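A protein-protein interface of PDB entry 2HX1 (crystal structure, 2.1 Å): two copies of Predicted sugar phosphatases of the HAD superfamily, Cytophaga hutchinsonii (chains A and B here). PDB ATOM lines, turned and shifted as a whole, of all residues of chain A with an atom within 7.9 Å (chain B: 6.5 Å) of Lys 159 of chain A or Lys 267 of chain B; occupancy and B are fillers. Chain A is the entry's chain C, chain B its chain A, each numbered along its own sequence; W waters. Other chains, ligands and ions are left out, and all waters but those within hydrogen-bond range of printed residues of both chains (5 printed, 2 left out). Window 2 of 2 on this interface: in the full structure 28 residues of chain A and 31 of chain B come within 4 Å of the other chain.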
ATOM      1  N   ASP A 126     -22.668  -6.978 -21.165  1.00  0.00           N
ATOM      2  CA  ASP A 126     -21.893  -7.631 -22.210  1.00  0.00           C
ATOM      3  C   ASP A 126     -20.711  -8.411 -21.611  1.00  0.00           C
ATOM      4  O   ASP A 126     -20.497  -8.432 -20.367  1.00  0.00           O
ATOM      5  CB  ASP A 126     -21.467  -6.606 -23.286  1.00  0.00           C
ATOM      6  CG  ASP A 126     -20.464  -5.563 -22.782  1.00  0.00           C
ATOM      7  OD1 ASP A 126     -19.794  -5.814 -21.772  1.00  0.00           O
ATOM      8  OD2 ASP A 126     -20.326  -4.480 -23.405  1.00  0.00           O
ATOM      9  N   ASP A 127     -19.941  -9.047 -22.504  1.00  0.00           N
ATOM     10  CA  ASP A 127     -18.782  -9.855 -22.110  1.00  0.00           C
ATOM     11  C   ASP A 127     -17.816  -9.089 -21.233  1.00  0.00           C
ATOM     12  O   ASP A 127     -17.217  -9.653 -20.327  1.00  0.00           O
ATOM     13  CB  ASP A 127     -18.050 -10.371 -23.343  1.00  0.00           C
ATOM     14  CG  ASP A 127     -18.797 -11.510 -24.051  1.00  0.00           C
ATOM     15  OD1 ASP A 127     -19.781 -12.048 -23.483  1.00  0.00           O
ATOM     16  OD2 ASP A 127     -18.383 -11.856 -25.181  1.00  0.00           O
ATOM     17  N   ILE A 130     -19.970  -8.351 -17.689  1.00  0.00           N
ATOM     18  CA  ILE A 130     -20.774  -9.395 -17.038  1.00  0.00           C
ATOM     19  C   ILE A 130     -20.068  -9.810 -15.754  1.00  0.00           C
ATOM     20  O   ILE A 130     -20.705 -10.121 -14.738  1.00  0.00           O
ATOM     21  CB  ILE A 130     -21.021 -10.628 -17.945  1.00  0.00           C
ATOM     22  CG1 ILE A 130     -22.002 -11.592 -17.286  1.00  0.00           C
ATOM     23  CG2 ILE A 130     -19.708 -11.373 -18.249  1.00  0.00           C
ATOM     24  CD1 ILE A 130     -22.509 -12.640 -18.209  1.00  0.00           C
ATOM     25  N   LYS A 152     -31.383 -12.618 -22.986  1.00  0.00           N
ATOM     26  CA  LYS A 152     -30.144 -12.135 -22.336  1.00  0.00           C
ATOM     27  C   LYS A 152     -30.156 -12.466 -20.836  1.00  0.00           C
ATOM     28  O   LYS A 152     -29.097 -12.795 -20.251  1.00  0.00           O
ATOM     29  CB  LYS A 152     -29.924 -10.628 -22.592  1.00  0.00           C
ATOM     30  CG  LYS A 152     -28.529 -10.101 -22.225  1.00  0.00           C
ATOM     31  CD  LYS A 152     -28.253  -8.641 -22.743  1.00  0.00           C
ATOM     32  CE  LYS A 152     -27.919  -8.607 -24.254  1.00  0.00           C
ATOM     33  NZ  LYS A 152     -28.314  -7.339 -24.995  1.00  0.00           N
ATOM     34  N   THR A 153     -31.343 -12.463 -20.215  1.00  0.00           N
ATOM     35  CA  THR A 153     -31.421 -12.758 -18.762  1.00  0.00           C
ATOM     36  C   THR A 153     -31.099 -14.221 -18.500  1.00  0.00           C
ATOM     37  O   THR A 153     -30.284 -14.530 -17.627  1.00  0.00           O
ATOM     38  CB  THR A 153     -32.772 -12.412 -18.145  1.00  0.00           C
ATOM     39  OG1 THR A 153     -32.987 -11.017 -18.271  1.00  0.00           O
ATOM     40  CG2 THR A 153     -32.790 -12.754 -16.657  1.00  0.00           C
ATOM     41  N   VAL A 154     -31.691 -15.091 -19.307  1.00  0.00           N
ATOM     42  CA  VAL A 154     -31.443 -16.537 -19.284  1.00  0.00           C
ATOM     43  C   VAL A 154     -29.964 -16.828 -19.432  1.00  0.00           C
ATOM     44  O   VAL A 154     -29.405 -17.585 -18.662  1.00  0.00           O
ATOM     45  CB  VAL A 154     -32.221 -17.254 -20.425  1.00  0.00           C
ATOM     46  CG1 VAL A 154     -31.672 -18.730 -20.697  1.00  0.00           C
ATOM     47  CG2 VAL A 154     -33.702 -17.227 -20.147  1.00  0.00           C
ATOM     48  N   ASN A 155     -29.315 -16.192 -20.400  1.00  0.00           N
ATOM     49  CA  ASN A 155     -27.858 -16.372 -20.564  1.00  0.00           C
ATOM     50  C   ASN A 155     -27.043 -15.799 -19.386  1.00  0.00           C
ATOM     51  O   ASN A 155     -26.079 -16.412 -18.940  1.00  0.00           O
ATOM     52  CB  ASN A 155     -27.415 -15.737 -21.877  1.00  0.00           C
ATOM     53  CG  ASN A 155     -27.830 -16.559 -23.098  1.00  0.00           C
ATOM     54  OD1 ASN A 155     -27.367 -17.670 -23.252  1.00  0.00           O
ATOM     55  ND2 ASN A 155     -28.676 -15.993 -23.987  1.00  0.00           N
ATOM     56  N   LEU A 156     -27.426 -14.622 -18.904  1.00  0.00           N
ATOM     57  CA  LEU A 156     -26.739 -13.983 -17.795  1.00  0.00           C
ATOM     58  C   LEU A 156     -26.689 -14.935 -16.586  1.00  0.00           C
ATOM     59  O   LEU A 156     -25.646 -15.111 -15.992  1.00  0.00           O
ATOM     60  CB  LEU A 156     -27.431 -12.676 -17.416  1.00  0.00           C
ATOM     61  CG  LEU A 156     -27.067 -12.093 -16.037  1.00  0.00           C
ATOM     62  CD1 LEU A 156     -25.615 -11.682 -15.981  1.00  0.00           C
ATOM     63  CD2 LEU A 156     -27.995 -10.919 -15.688  1.00  0.00           C
ATOM     64  N   LEU A 157     -27.831 -15.542 -16.268  1.00  0.00           N
ATOM     65  CA  LEU A 157     -27.966 -16.405 -15.114  1.00  0.00           C
ATOM     66  C   LEU A 157     -27.336 -17.771 -15.331  1.00  0.00           C
ATOM     67  O   LEU A 157     -26.956 -18.436 -14.363  1.00  0.00           O
ATOM     68  CB  LEU A 157     -29.431 -16.589 -14.726  1.00  0.00           C
ATOM     69  CG  LEU A 157     -30.137 -15.362 -14.173  1.00  0.00           C
ATOM     70  CD1 LEU A 157     -31.625 -15.641 -14.093  1.00  0.00           C
ATOM     71  CD2 LEU A 157     -29.584 -14.997 -12.795  1.00  0.00           C
ATOM     72  N   ARG A 158     -27.236 -18.208 -16.581  1.00  0.00           N
ATOM     73  CA  ARG A 158     -26.454 -19.401 -16.906  1.00  0.00           C
ATOM     74  C   ARG A 158     -24.956 -19.161 -16.746  1.00  0.00           C
ATOM     75  O   ARG A 158     -24.230 -20.087 -16.420  1.00  0.00           O
ATOM     76  CB  ARG A 158     -26.699 -19.871 -18.340  1.00  0.00           C
ATOM     77  CG  ARG A 158     -28.023 -20.587 -18.590  1.00  0.00           C
ATOM     78  CD  ARG A 158     -28.279 -20.724 -20.084  1.00  0.00           C
ATOM     79  NE  ARG A 158     -27.303 -21.610 -20.731  1.00  0.00           N
ATOM     80  CZ  ARG A 158     -26.256 -21.226 -21.468  1.00  0.00           C
ATOM     81  NH1 ARG A 158     -25.968 -19.925 -21.701  1.00  0.00           N
ATOM     82  NH2 ARG A 158     -25.478 -22.180 -21.986  1.00  0.00           N
ATOM     83  N   LYS A 159     -24.496 -17.937 -16.959  1.00  0.00           N
ATOM     84  CA  LYS A 159     -23.064 -17.660 -16.972  1.00  0.00           C
ATOM     85  C   LYS A 159     -22.514 -17.140 -15.663  1.00  0.00           C
ATOM     86  O   LYS A 159     -21.340 -17.265 -15.423  1.00  0.00           O
ATOM     87  CB  LYS A 159     -22.753 -16.654 -18.058  1.00  0.00           C
ATOM     88  CG  LYS A 159     -22.934 -17.169 -19.492  1.00  0.00           C
ATOM     89  CD  LYS A 159     -22.851 -15.989 -20.439  1.00  0.00           C
ATOM     90  CE  LYS A 159     -23.155 -16.331 -21.867  1.00  0.00           C
ATOM     91  NZ  LYS A 159     -22.803 -15.187 -22.756  1.00  0.00           N
ATOM     92  N   ARG A 160     -23.335 -16.520 -14.841  1.00  0.00           N
ATOM     93  CA  ARG A 160     -22.839 -15.799 -13.680  1.00  0.00           C
ATOM     94  C   ARG A 160     -23.472 -16.369 -12.419  1.00  0.00           C
ATOM     95  O   ARG A 160     -24.673 -16.623 -12.392  1.00  0.00           O
ATOM     96  CB  ARG A 160     -23.210 -14.350 -13.926  1.00  0.00           C
ATOM     97  CG  ARG A 160     -22.547 -13.399 -13.088  1.00  0.00           C
ATOM     98  CD  ARG A 160     -21.117 -13.089 -13.466  1.00  0.00           C
ATOM     99  NE  ARG A 160     -20.633 -12.319 -12.332  1.00  0.00           N
ATOM    100  CZ  ARG A 160     -20.123 -12.845 -11.226  1.00  0.00           C
ATOM    101  NH1 ARG A 160     -19.933 -14.158 -11.130  1.00  0.00           N
ATOM    102  NH2 ARG A 160     -19.782 -12.046 -10.224  1.00  0.00           N
ATOM    103  N   THR A 161     -22.653 -16.630 -11.403  1.00  0.00           N
ATOM    104  CA  THR A 161     -23.134 -17.031 -10.080  1.00  0.00           C
ATOM    105  C   THR A 161     -23.543 -15.772  -9.311  1.00  0.00           C
ATOM    106  O   THR A 161     -22.718 -15.122  -8.644  1.00  0.00           O
ATOM    107  CB  THR A 161     -22.035 -17.838  -9.320  1.00  0.00           C
ATOM    108  OG1 THR A 161     -21.748 -19.022 -10.066  1.00  0.00           O
ATOM    109  CG2 THR A 161     -22.464 -18.228  -7.912  1.00  0.00           C
ATOM    110  N   ILE A 162     -24.820 -15.400  -9.472  1.00  0.00           N
ATOM    111  CA  ILE A 162     -25.394 -14.239  -8.809  1.00  0.00           C
ATOM    112  C   ILE A 162     -26.789 -14.521  -8.272  1.00  0.00           C
ATOM    113  O   ILE A 162     -27.494 -15.389  -8.798  1.00  0.00           O
ATOM    114  CB  ILE A 162     -25.476 -13.046  -9.756  1.00  0.00           C
ATOM    115  CG1 ILE A 162     -26.282 -13.383 -11.013  1.00  0.00           C
ATOM    116  CG2 ILE A 162     -24.060 -12.609 -10.137  1.00  0.00           C
ATOM    117  CD1 ILE A 162     -26.352 -12.253 -11.975  1.00  0.00           C
ATOM    118  N   PRO A 163     -27.183 -13.808  -7.204  1.00  0.00           N
ATOM    119  CA  PRO A 163     -28.589 -13.866  -6.810  1.00  0.00           C
ATOM    120  C   PRO A 163     -29.499 -13.222  -7.849  1.00  0.00           C
ATOM    121  O   PRO A 163     -29.164 -12.197  -8.423  1.00  0.00           O
ATOM    122  CB  PRO A 163     -28.628 -13.076  -5.489  1.00  0.00           C
ATOM    123  CG  PRO A 163     -27.439 -12.167  -5.540  1.00  0.00           C
ATOM    124  CD  PRO A 163     -26.378 -12.957  -6.305  1.00  0.00           C
ATOM    125  N   LEU A 195     -35.165 -22.299 -16.504  1.00  0.00           N
ATOM    126  CA  LEU A 195     -33.939 -22.545 -15.752  1.00  0.00           C
ATOM    127  C   LEU A 195     -34.119 -23.429 -14.524  1.00  0.00           C
ATOM    128  O   LEU A 195     -33.128 -23.873 -13.954  1.00  0.00           O
ATOM    129  CB  LEU A 195     -33.388 -21.208 -15.274  1.00  0.00           C
ATOM    130  CG  LEU A 195     -32.881 -20.195 -16.304  1.00  0.00           C
ATOM    131  CD1 LEU A 195     -32.466 -18.928 -15.575  1.00  0.00           C
ATOM    132  CD2 LEU A 195     -31.739 -20.748 -17.089  1.00  0.00           C
ATOM    133  N   ARG A 198     -34.910 -20.412  -9.013  1.00  0.00           N
ATOM    134  CA  ARG A 198     -33.698 -19.636  -9.182  1.00  0.00           C
ATOM    135  C   ARG A 198     -33.806 -18.272  -8.512  1.00  0.00           C
ATOM    136  O   ARG A 198     -32.766 -17.618  -8.299  1.00  0.00           O
ATOM    137  CB  ARG A 198     -33.442 -19.499 -10.713  1.00  0.00           C
ATOM    138  CG  ARG A 198     -32.204 -18.708 -11.152  1.00  0.00           C
ATOM    139  CD  ARG A 198     -30.938 -19.438 -10.880  1.00  0.00           C
ATOM    140  NE  ARG A 198     -29.771 -18.707 -11.368  1.00  0.00           N
ATOM    141  CZ  ARG A 198     -29.214 -17.671 -10.755  1.00  0.00           C
ATOM    142  NH1 ARG A 198     -29.711 -17.196  -9.637  1.00  0.00           N
ATOM    143  NH2 ARG A 198     -28.148 -17.098 -11.280  1.00  0.00           N
ATOM    144  N   ALA B 262     -20.302 -28.248  -5.028  1.00  0.00           N
ATOM    145  CA  ALA B 262     -20.617 -26.947  -4.444  1.00  0.00           C
ATOM    146  C   ALA B 262     -20.689 -25.829  -5.473  1.00  0.00           C
ATOM    147  O   ALA B 262     -21.628 -25.034  -5.469  1.00  0.00           O
ATOM    148  CB  ALA B 262     -19.623 -26.593  -3.357  1.00  0.00           C
ATOM    149  N   GLU B 263     -19.691 -25.743  -6.348  1.00  0.00           N
ATOM    150  CA  GLU B 263     -19.659 -24.631  -7.293  1.00  0.00           C
ATOM    151  C   GLU B 263     -20.856 -24.695  -8.229  1.00  0.00           C
ATOM    152  O   GLU B 263     -21.560 -23.698  -8.480  1.00  0.00           O
ATOM    153  CB  GLU B 263     -18.363 -24.608  -8.092  1.00  0.00           C
ATOM    154  CG  GLU B 263     -17.219 -23.959  -7.361  1.00  0.00           C
ATOM    155  CD  GLU B 263     -16.154 -23.385  -8.298  1.00  0.00           C
ATOM    156  OE1 GLU B 263     -16.420 -22.340  -8.960  1.00  0.00           O
ATOM    157  OE2 GLU B 263     -15.049 -23.972  -8.340  1.00  0.00           O
ATOM    158  N   THR B 264     -21.120 -25.890  -8.694  1.00  0.00           N
ATOM    159  CA  THR B 264     -22.274 -26.124  -9.560  1.00  0.00           C
ATOM    160  C   THR B 264     -23.595 -25.792  -8.857  1.00  0.00           C
ATOM    161  O   THR B 264     -24.425 -25.054  -9.405  1.00  0.00           O
ATOM    162  CB  THR B 264     -22.242 -27.559 -10.124  1.00  0.00           C
ATOM    163  OG1 THR B 264     -21.281 -27.580 -11.186  1.00  0.00           O
ATOM    164  CG2 THR B 264     -23.589 -27.988 -10.661  1.00  0.00           C
ATOM    165  N   LYS B 265     -23.787 -26.286  -7.637  1.00  0.00           N
ATOM    166  CA  LYS B 265     -25.048 -26.012  -6.952  1.00  0.00           C
ATOM    167  C   LYS B 265     -25.159 -24.530  -6.656  1.00  0.00           C
ATOM    168  O   LYS B 265     -26.246 -23.966  -6.787  1.00  0.00           O
ATOM    169  CB  LYS B 265     -25.227 -26.860  -5.704  1.00  0.00           C
ATOM    170  CG  LYS B 265     -25.422 -28.354  -5.995  1.00  0.00           C
ATOM    171  CD  LYS B 265     -25.393 -29.162  -4.686  1.00  0.00           C
ATOM    172  CE  LYS B 265     -26.072 -30.535  -4.820  1.00  0.00           C
ATOM    173  NZ  LYS B 265     -26.351 -31.135  -3.493  1.00  0.00           N
ATOM    174  N   ILE B 266     -24.048 -23.877  -6.296  1.00  0.00           N
ATOM    175  CA  ILE B 266     -24.103 -22.458  -5.991  1.00  0.00           C
ATOM    176  C   ILE B 266     -24.482 -21.665  -7.263  1.00  0.00           C
ATOM    177  O   ILE B 266     -25.345 -20.777  -7.225  1.00  0.00           O
ATOM    178  CB  ILE B 266     -22.804 -21.966  -5.335  1.00  0.00           C
ATOM    179  CG1 ILE B 266     -22.669 -22.593  -3.941  1.00  0.00           C
ATOM    180  CG2 ILE B 266     -22.772 -20.429  -5.235  1.00  0.00           C
ATOM    181  CD1 ILE B 266     -21.269 -22.514  -3.337  1.00  0.00           C
ATOM    182  N   LYS B 267     -23.877 -22.033  -8.388  1.00  0.00           N
ATOM    183  CA  LYS B 267     -24.137 -21.387  -9.672  1.00  0.00           C
ATOM    184  C   LYS B 267     -25.550 -21.635 -10.174  1.00  0.00           C
ATOM    185  O   LYS B 267     -26.177 -20.727 -10.724  1.00  0.00           O
ATOM    186  CB  LYS B 267     -23.125 -21.863 -10.724  1.00  0.00           C
ATOM    187  CG  LYS B 267     -23.145 -21.073 -12.041  1.00  0.00           C
ATOM    188  CD  LYS B 267     -21.848 -21.310 -12.869  1.00  0.00           C
ATOM    189  CE  LYS B 267     -21.986 -20.786 -14.300  1.00  0.00           C
ATOM    190  NZ  LYS B 267     -20.689 -20.666 -15.061  1.00  0.00           N
ATOM    191  N   SER B 268     -26.051 -22.859 -10.008  1.00  0.00           N
ATOM    192  CA  SER B 268     -27.390 -23.199 -10.527  1.00  0.00           C
ATOM    193  C   SER B 268     -28.530 -22.580  -9.699  1.00  0.00           C
ATOM    194  O   SER B 268     -29.577 -22.232 -10.239  1.00  0.00           O
ATOM    195  CB  SER B 268     -27.520 -24.711 -10.693  1.00  0.00           C
ATOM    196  OG  SER B 268     -27.915 -25.306  -9.493  1.00  0.00           O
ATOM    197  N   THR B 269     -28.314 -22.370  -8.404  1.00  0.00           N
ATOM    198  CA  THR B 269     -29.336 -21.763  -7.534  1.00  0.00           C
ATOM    199  C   THR B 269     -29.144 -20.248  -7.361  1.00  0.00           C
ATOM    200  O   THR B 269     -30.102 -19.508  -7.055  1.00  0.00           O
ATOM    201  CB  THR B 269     -29.338 -22.403  -6.120  1.00  0.00           C
ATOM    202  OG1 THR B 269     -28.081 -22.172  -5.491  1.00  0.00           O
ATOM    203  CG2 THR B 269     -29.593 -23.909  -6.155  1.00  0.00           C
ATOM    204  N   GLY B 270     -27.924 -19.774  -7.562  1.00  0.00           N
ATOM    205  CA  GLY B 270     -27.603 -18.386  -7.255  1.00  0.00           C
ATOM    206  C   GLY B 270     -27.653 -18.064  -5.766  1.00  0.00           C
ATOM    207  O   GLY B 270     -27.727 -16.882  -5.348  1.00  0.00           O
ATOM    208  N   ILE B 271     -27.596 -19.114  -4.954  1.00  0.00           N
ATOM    209  CA  ILE B 271     -27.552 -18.954  -3.513  1.00  0.00           C
ATOM    210  C   ILE B 271     -26.087 -18.952  -3.082  1.00  0.00           C
ATOM    211  O   ILE B 271     -25.449 -20.010  -3.008  1.00  0.00           O
ATOM    212  CB  ILE B 271     -28.319 -20.078  -2.775  1.00  0.00           C
ATOM    213  CG1 ILE B 271     -29.809 -20.061  -3.157  1.00  0.00           C
ATOM    214  CG2 ILE B 271     -28.148 -19.917  -1.241  1.00  0.00           C
ATOM    215  CD1 ILE B 271     -30.575 -21.379  -2.824  1.00  0.00           C
HETATM  216  O   HOH W   1     -30.994 -16.623  -7.003  1.00  0.00           O
HETATM  217  O   HOH W   2     -30.521 -23.113 -12.985  1.00  0.00           O
HETATM  218  O   HOH W   3     -20.449 -21.417  -8.739  1.00  0.00           O
HETATM  219  O   HOH W   4     -19.833 -19.116 -17.062  1.00  0.00           O
HETATM  220  O   HOH W   5     -32.176 -24.134 -10.661  1.00  0.00           O
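Among the printed residues, merely in contact across the chains: Arg 158 of chain A with Lys 267 of chain B (3.2 Å), Thr 161 of chain A with Ile 266 of chain B (3.5 Å), Thr 161 of chain A with Lys 267 of chain B (3.2 Å), Ile 162 of chain A with Gly 270 of chain B (3.4 Å), Pro 163 of chain A with Gly 270 of chain B (3.5 Å), Arg 198 of chain A with Ser 268 of chain B (3.2 Å) and Arg 198 of chain A with Gly 270 of chain B (3.4 Å).
No position is printed for both chains.
Water W1 lies within hydrogen-bond range of the backbone carbonyl oxygen of Arg 198 of chain A (2.4 Å) and the backbone carbonyl oxygen of Thr 269 of chain B (3.0 Å).
Water W4 bridges NZ of Lys 267 of chain B (2.7 Å) and O of Lys 159 of chain A (2.9 Å).
Water W2 lies within hydrogen-bond range of the backbone carbonyl oxygen (O) of Leu 195 of chain A (2.9 Å) and the backbone carbonyl oxygen (O) of Ser 268 of chain B (3.0 Å).
Water W5 bridges the backbone carbonyl oxygen of Ser 268 of chain B (3.2 Å) and the backbone carbonyl oxygen of Leu 195 of chain A (3.4 Å).
O of Lys 265 of chain B sits at hydrogen-bond distance from OG1 of Thr 269 of chain B.
The backbone carbonyl oxygen (O) of Lys 265 of chain B lies within hydrogen-bond range of the side-chain hydroxyl (OG) of Ser 268 of chain B (3.5 Å).
The side-chain amide oxygen (OD1) of Asn 155 of chain A is in hydrogen-bond range of the guanidinium group (NH1) of Arg 158 of chain A (3.1 Å).
The guanidinium group (NH1) of Arg 198 of chain A lies within hydrogen-bond range of the backbone carbonyl oxygen (O) of Ile 162 of chain A (3.0 Å).
The side-chain hydroxyl of Thr 269 of chain B lies close to the backbone NH of Ile 271 of chain B, at 3.1 Å.
NH1 of Arg 198 of chain A lies within hydrogen-bond range of O of Thr 269 of chain B (3.5 Å).
The side-chain amino group of Lys 267 of chain B lies within hydrogen-bond range of the backbone carbonyl oxygen of Lys 159 of chain A (3.5 Å).
Of the 10 printed residues of chain B, 5 touch a printed residue of chain A.
Printed residues of chain B that touch a printed residue of chain A: Ile 266, Lys 267, Ser 268, Thr 269 and Gly 270.
Hydrophobic or aromatic side chains of chain B within 4 Å of the printed part of chain A: Ile 266.
Hydrophobic or aromatic side chains of chain A within 4 Å of the printed part of chain B: Pro 163.
Along chain A the printed residues that touch a printed residue of chain B span positions 158 to 198.
Among the printed residues, no Asp or Glu carboxylate lies within 4 Å of a Lys or Arg side-chain nitrogen of the other chain.
Of the printed residues of chain B, Lys 159 of chain A touches Lys 267.
Lys 267 of chain B touches just these residues of chain A: Arg 158, Lys 159 and Thr 161.
Of the printed residues of chain B, Thr 161 of chain A touches Ile 266 (3.5 Å) and Lys 267 (3.2 Å).
Printed residues of chain A within 4 Å of Ser 268 of chain B: Arg 198 (3.2 Å).
Of the printed residues of chain B, Arg 158 of chain A touches Lys 267.
Of the printed residues of chain A, Gly 270 of chain B touches Ile 162 (3.4 Å), Pro 163 (3.5 Å) and Arg 198 (3.4 Å).
Printed residues of chain B within 4 Å of Ile 162 of chain A: Gly 270.
The nearest printed residue of chain B that does not touch Thr 161 of chain A is Glu 263 of chain B (4.9 Å).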
